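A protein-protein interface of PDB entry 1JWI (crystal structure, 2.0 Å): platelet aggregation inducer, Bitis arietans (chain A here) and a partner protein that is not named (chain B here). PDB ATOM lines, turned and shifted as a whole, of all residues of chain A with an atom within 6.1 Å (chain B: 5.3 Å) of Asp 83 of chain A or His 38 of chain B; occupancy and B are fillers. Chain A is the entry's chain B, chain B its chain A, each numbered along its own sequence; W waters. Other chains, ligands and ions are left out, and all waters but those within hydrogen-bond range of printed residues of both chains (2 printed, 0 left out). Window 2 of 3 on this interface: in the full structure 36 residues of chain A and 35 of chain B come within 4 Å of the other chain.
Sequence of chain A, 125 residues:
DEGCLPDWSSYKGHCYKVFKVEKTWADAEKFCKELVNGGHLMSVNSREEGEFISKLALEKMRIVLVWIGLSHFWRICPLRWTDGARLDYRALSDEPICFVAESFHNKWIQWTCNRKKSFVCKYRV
Water W1 lies within hydrogen-bond range of the backbone carbonyl oxygen of Leu 39 of chain B (2.7 Å), the backbone NH of Asp 83 of chain A (3.1 Å) and the backbone NH of Thr 82 of chain A (3.2 Å).
Water W2 lies within hydrogen-bond range of OD1 of Asp 83 of chain A (2.9 Å), O of Leu 39 of chain B (3.0 Å) and N of Ser 41 of chain B (3.4 Å).
Of the printed residues of chain B, Thr 82 of chain A touches Glu 29, His 38 and Leu 39.
Of chain B, only His 38 (3.7 Å) and Ser 41 (2.6 Å) come within 4 Å of Asp 83 of chain A.
Of the printed residues of chain A, Glu 29 of chain B touches Thr 82 (3.0 Å).
Of chain A, only Thr 82 and Asp 83 come within 4 Å of His 38 of chain B.
The nearest printed residue of chain A that does not touch His 38 of chain B is Gly 84 of chain A (6.3 Å).
The nearest printed residue of chain B that does not touch Trp 81 of chain A is Leu 39 of chain B (5.6 Å).
OG1 of Thr 82 of chain A is in hydrogen-bond range of OE1 of Glu 29 of chain B (3.1 Å).
The side-chain hydroxyl of Ser 41 of chain B sits at hydrogen-bond distance from the side-chain carboxylate of Asp 83 of chain A, at 2.6 Å.
Of the 6 printed residues of chain A, 3 touch a printed residue of chain B.
Among the printed residues, 7 pairs touch across the chains.
Among the printed residues, pairs that only touch across the chains: Trp 81 of chain A with Ala 40 of chain B (3.4 Å), Trp 81 of chain A with Ser 41 of chain B (3.5 Å), Thr 82 of chain A with His 38 of chain B (3.4 Å), Thr 82 of chain A with Leu 39 of chain B (3.7 Å) and Asp 83 of chain A with His 38 of chain B (3.7 Å).
N of Ala 40 of chain B is in hydrogen-bond range of O of Ile 124 of chain B (2.9 Å).
The side-chain sulfur of Cys 32 of chain B sits close to the backbone NH of Leu 39 of chain B (3.8 Å).
O of His 38 of chain B is in hydrogen-bond range of N of Lys 126 of chain B, 2.9 Å away.
N of Leu 39 of chain B sits at hydrogen-bond distance from OE2 of Glu 29 of chain B (2.9 Å).
The backbone NH (N) of Ala 85 of chain A lies within hydrogen-bond range of the side-chain carboxylate (OD2) of Asp 83 of chain A.
A ring nitrogen (ND1) of His 38 of chain B lies within hydrogen-bond range of the side-chain carboxylate (OE1) of Glu 29 of chain B (2.7 Å).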
ATOM      1  N   TRP A  81      15.024 -15.776  19.433  1.00  0.00           N
ATOM      2  CA  TRP A  81      15.134 -14.921  18.258  1.00  0.00           C
ATOM      3  C   TRP A  81      13.829 -15.087  17.495  1.00  0.00           C
ATOM      4  O   TRP A  81      13.286 -16.190  17.390  1.00  0.00           O
ATOM      5  CB  TRP A  81      16.292 -15.340  17.354  1.00  0.00           C
ATOM      6  CG  TRP A  81      17.635 -14.951  17.861  1.00  0.00           C
ATOM      7  CD1 TRP A  81      18.651 -15.793  18.205  1.00  0.00           C
ATOM      8  CD2 TRP A  81      18.126 -13.618  18.058  1.00  0.00           C
ATOM      9  NE1 TRP A  81      19.747 -15.068  18.605  1.00  0.00           N
ATOM     10  CE2 TRP A  81      19.455 -13.731  18.526  1.00  0.00           C
ATOM     11  CE3 TRP A  81      17.574 -12.341  17.887  1.00  0.00           C
ATOM     12  CZ2 TRP A  81      20.247 -12.610  18.825  1.00  0.00           C
ATOM     13  CZ3 TRP A  81      18.359 -11.224  18.184  1.00  0.00           C
ATOM     14  CH2 TRP A  81      19.683 -11.370  18.650  1.00  0.00           C
ATOM     15  N   THR A  82      13.341 -13.989  16.948  1.00  0.00           N
ATOM     16  CA  THR A  82      12.096 -13.991  16.219  1.00  0.00           C
ATOM     17  C   THR A  82      12.156 -14.882  14.967  1.00  0.00           C
ATOM     18  O   THR A  82      11.120 -15.308  14.444  1.00  0.00           O
ATOM     19  CB  THR A  82      11.744 -12.535  15.855  1.00  0.00           C
ATOM     20  OG1 THR A  82      10.327 -12.352  15.911  1.00  0.00           O
ATOM     21  CG2 THR A  82      12.277 -12.177  14.486  1.00  0.00           C
ATOM     22  N   ASP A  83      13.366 -15.180  14.495  1.00  0.00           N
ATOM     23  CA  ASP A  83      13.523 -16.008  13.305  1.00  0.00           C
ATOM     24  C   ASP A  83      13.813 -17.482  13.606  1.00  0.00           C
ATOM     25  O   ASP A  83      14.113 -18.253  12.702  1.00  0.00           O
ATOM     26  CB  ASP A  83      14.620 -15.432  12.392  1.00  0.00           C
ATOM     27  CG  ASP A  83      15.984 -15.401  13.054  1.00  0.00           C
ATOM     28  OD1 ASP A  83      16.943 -14.890  12.425  1.00  0.00           O
ATOM     29  OD2 ASP A  83      16.102 -15.888  14.198  1.00  0.00           O
ATOM     30  N   GLY A  84      13.724 -17.870  14.873  1.00  0.00           N
ATOM     31  CA  GLY A  84      13.967 -19.254  15.238  1.00  0.00           C
ATOM     32  C   GLY A  84      15.418 -19.628  15.481  1.00  0.00           C
ATOM     33  O   GLY A  84      15.704 -20.681  16.049  1.00  0.00           O
ATOM     34  N   ALA A  85      16.341 -18.778  15.046  1.00  0.00           N
ATOM     35  CA  ALA A  85      17.757 -19.057  15.236  1.00  0.00           C
ATOM     36  C   ALA A  85      18.042 -19.348  16.706  1.00  0.00           C
ATOM     37  O   ALA A  85      17.294 -18.933  17.592  1.00  0.00           O
ATOM     38  CB  ALA A  85      18.595 -17.873  14.762  1.00  0.00           C
ATOM     39  N   ARG A  86      19.121 -20.076  16.957  1.00  0.00           N
ATOM     40  CA  ARG A  86      19.515 -20.411  18.317  1.00  0.00           C
ATOM     41  C   ARG A  86      20.303 -19.250  18.897  1.00  0.00           C
ATOM     42  O   ARG A  86      20.997 -18.538  18.166  1.00  0.00           O
ATOM     43  CB  ARG A  86      20.380 -21.677  18.321  1.00  0.00           C
ATOM     44  CG  ARG A  86      19.584 -22.977  18.379  1.00  0.00           C
ATOM     45  CD  ARG A  86      19.384 -23.429  19.821  1.00  0.00           C
ATOM     46  NE  ARG A  86      20.644 -23.853  20.429  1.00  0.00           N
ATOM     47  CZ  ARG A  86      20.791 -24.171  21.712  1.00  0.00           C
ATOM     48  NH1 ARG A  86      19.755 -24.113  22.541  1.00  0.00           N
ATOM     49  NH2 ARG A  86      21.978 -24.547  22.169  1.00  0.00           N
ATOM     50  N   GLU B  29       8.643  -6.009  14.021  1.00  0.00           N
ATOM     51  CA  GLU B  29       8.747  -7.369  13.496  1.00  0.00           C
ATOM     52  C   GLU B  29       7.800  -7.578  12.312  1.00  0.00           C
ATOM     53  O   GLU B  29       8.185  -8.162  11.299  1.00  0.00           O
ATOM     54  CB  GLU B  29       8.430  -8.389  14.599  1.00  0.00           C
ATOM     55  CG  GLU B  29       8.236  -9.823  14.108  1.00  0.00           C
ATOM     56  CD  GLU B  29       9.503 -10.451  13.566  1.00  0.00           C
ATOM     57  OE1 GLU B  29       9.429 -11.600  13.066  1.00  0.00           O
ATOM     58  OE2 GLU B  29      10.576  -9.810  13.645  1.00  0.00           O
ATOM     59  N   CYS B  32       9.122  -5.987   9.174  1.00  0.00           N
ATOM     60  CA  CYS B  32      10.220  -6.764   8.610  1.00  0.00           C
ATOM     61  C   CYS B  32       9.650  -7.983   7.885  1.00  0.00           C
ATOM     62  O   CYS B  32      10.116  -8.349   6.797  1.00  0.00           O
ATOM     63  CB  CYS B  32      11.180  -7.247   9.707  1.00  0.00           C
ATOM     64  SG  CYS B  32      12.239  -5.987  10.502  1.00  0.00           S
ATOM     65  N   VAL B  33       8.658  -8.622   8.504  1.00  0.00           N
ATOM     66  CA  VAL B  33       8.015  -9.789   7.911  1.00  0.00           C
ATOM     67  C   VAL B  33       7.474  -9.372   6.541  1.00  0.00           C
ATOM     68  O   VAL B  33       7.721 -10.038   5.531  1.00  0.00           O
ATOM     69  CB  VAL B  33       6.850 -10.277   8.800  1.00  0.00           C
ATOM     70  CG1 VAL B  33       5.921 -11.194   8.018  1.00  0.00           C
ATOM     71  CG2 VAL B  33       7.406 -11.021  10.012  1.00  0.00           C
ATOM     72  N   SER B  36       9.667  -9.666   3.685  1.00  0.00           N
ATOM     73  CA  SER B  36      10.269 -10.988   3.571  1.00  0.00           C
ATOM     74  C   SER B  36      11.422 -11.238   4.537  1.00  0.00           C
ATOM     75  O   SER B  36      12.409 -11.872   4.171  1.00  0.00           O
ATOM     76  CB  SER B  36      10.748 -11.210   2.133  1.00  0.00           C
ATOM     77  OG  SER B  36      11.231 -12.528   1.961  1.00  0.00           O
ATOM     78  N   GLY B  37      11.297 -10.754   5.770  1.00  0.00           N
ATOM     79  CA  GLY B  37      12.358 -10.967   6.736  1.00  0.00           C
ATOM     80  C   GLY B  37      11.877 -11.019   8.172  1.00  0.00           C
ATOM     81  O   GLY B  37      10.758 -11.448   8.447  1.00  0.00           O
ATOM     82  N   HIS B  38      12.736 -10.578   9.086  1.00  0.00           N
ATOM     83  CA  HIS B  38      12.440 -10.549  10.520  1.00  0.00           C
ATOM     84  C   HIS B  38      13.358  -9.501  11.135  1.00  0.00           C
ATOM     85  O   HIS B  38      14.274  -9.011  10.474  1.00  0.00           O
ATOM     86  CB  HIS B  38      12.789 -11.893  11.183  1.00  0.00           C
ATOM     87  CG  HIS B  38      11.896 -13.030  10.795  1.00  0.00           C
ATOM     88  ND1 HIS B  38      10.591 -13.131  11.223  1.00  0.00           N
ATOM     89  CD2 HIS B  38      12.136 -14.137  10.051  1.00  0.00           C
ATOM     90  CE1 HIS B  38      10.066 -14.256  10.763  1.00  0.00           C
ATOM     91  NE2 HIS B  38      10.982 -14.883  10.050  1.00  0.00           N
ATOM     92  N   LEU B  39      13.110  -9.162  12.397  1.00  0.00           N
ATOM     93  CA  LEU B  39      13.991  -8.242  13.089  1.00  0.00           C
ATOM     94  C   LEU B  39      15.276  -9.051  13.084  1.00  0.00           C
ATOM     95  O   LEU B  39      15.236 -10.281  13.184  1.00  0.00           O
ATOM     96  CB  LEU B  39      13.520  -7.996  14.524  1.00  0.00           C
ATOM     97  CG  LEU B  39      12.406  -6.960  14.640  1.00  0.00           C
ATOM     98  CD1 LEU B  39      11.886  -6.900  16.072  1.00  0.00           C
ATOM     99  CD2 LEU B  39      12.951  -5.594  14.187  1.00  0.00           C
ATOM    100  N   ALA B  40      16.404  -8.368  12.952  1.00  0.00           N
ATOM    101  CA  ALA B  40      17.702  -9.022  12.894  1.00  0.00           C
ATOM    102  C   ALA B  40      18.038  -9.934  14.065  1.00  0.00           C
ATOM    103  O   ALA B  40      17.783  -9.610  15.227  1.00  0.00           O
ATOM    104  CB  ALA B  40      18.804  -7.965  12.747  1.00  0.00           C
ATOM    105  N   SER B  41      18.604 -11.088  13.735  1.00  0.00           N
ATOM    106  CA  SER B  41      19.065 -12.041  14.729  1.00  0.00           C
ATOM    107  C   SER B  41      20.567 -11.929  14.493  1.00  0.00           C
ATOM    108  O   SER B  41      20.986 -11.715  13.355  1.00  0.00           O
ATOM    109  CB  SER B  41      18.587 -13.453  14.403  1.00  0.00           C
ATOM    110  OG  SER B  41      19.211 -13.948  13.229  1.00  0.00           O
ATOM    111  N   ILE B 124      15.949  -2.742  12.860  1.00  0.00           N
ATOM    112  CA  ILE B 124      16.751  -3.350  11.818  1.00  0.00           C
ATOM    113  C   ILE B 124      16.192  -4.685  11.358  1.00  0.00           C
ATOM    114  O   ILE B 124      15.998  -5.602  12.159  1.00  0.00           O
ATOM    115  CB  ILE B 124      18.194  -3.560  12.311  1.00  0.00           C
ATOM    116  CG1 ILE B 124      18.996  -4.333  11.265  1.00  0.00           C
ATOM    117  CG2 ILE B 124      18.181  -4.309  13.637  1.00  0.00           C
ATOM    118  CD1 ILE B 124      20.371  -4.728  11.727  1.00  0.00           C
ATOM    119  N   CYS B 125      15.940  -4.776  10.054  1.00  0.00           N
ATOM    120  CA  CYS B 125      15.422  -5.991   9.444  1.00  0.00           C
ATOM    121  C   CYS B 125      16.551  -6.798   8.801  1.00  0.00           C
ATOM    122  O   CYS B 125      17.598  -6.258   8.427  1.00  0.00           O
ATOM    123  CB  CYS B 125      14.379  -5.652   8.378  1.00  0.00           C
ATOM    124  SG  CYS B 125      12.892  -4.806   8.992  1.00  0.00           S
ATOM    125  N   LYS B 126      16.321  -8.099   8.692  1.00  0.00           N
ATOM    126  CA  LYS B 126      17.275  -9.018   8.095  1.00  0.00           C
ATOM    127  C   LYS B 126      16.481 -10.054   7.298  1.00  0.00           C
ATOM    128  O   LYS B 126      15.494 -10.607   7.793  1.00  0.00           O
ATOM    129  CB  LYS B 126      18.089  -9.697   9.197  1.00  0.00           C
ATOM    130  CG  LYS B 126      18.955 -10.856   8.747  1.00  0.00           C
ATOM    131  CD  LYS B 126      19.666 -11.451   9.950  1.00  0.00           C
ATOM    132  CE  LYS B 126      20.429 -12.714   9.595  1.00  0.00           C
ATOM    133  NZ  LYS B 126      21.021 -13.341  10.815  1.00  0.00           N
ATOM    134  N   SER B 127      16.894 -10.297   6.058  1.00  0.00           N
ATOM    135  CA  SER B 127      16.215 -11.275   5.218  1.00  0.00           C
ATOM    136  C   SER B 127      17.229 -11.998   4.337  1.00  0.00           C
ATOM    137  O   SER B 127      18.336 -11.444   4.155  1.00  0.00           O
ATOM    138  CB  SER B 127      15.154 -10.590   4.352  1.00  0.00           C
ATOM    139  OG  SER B 127      15.740  -9.717   3.403  1.00  0.00           O
HETATM  140  O   HOH W   1      15.073 -12.548  14.699  1.00  0.00           O
HETATM  141  O   HOH W   2      16.541 -12.223  11.302  1.00  0.00           O
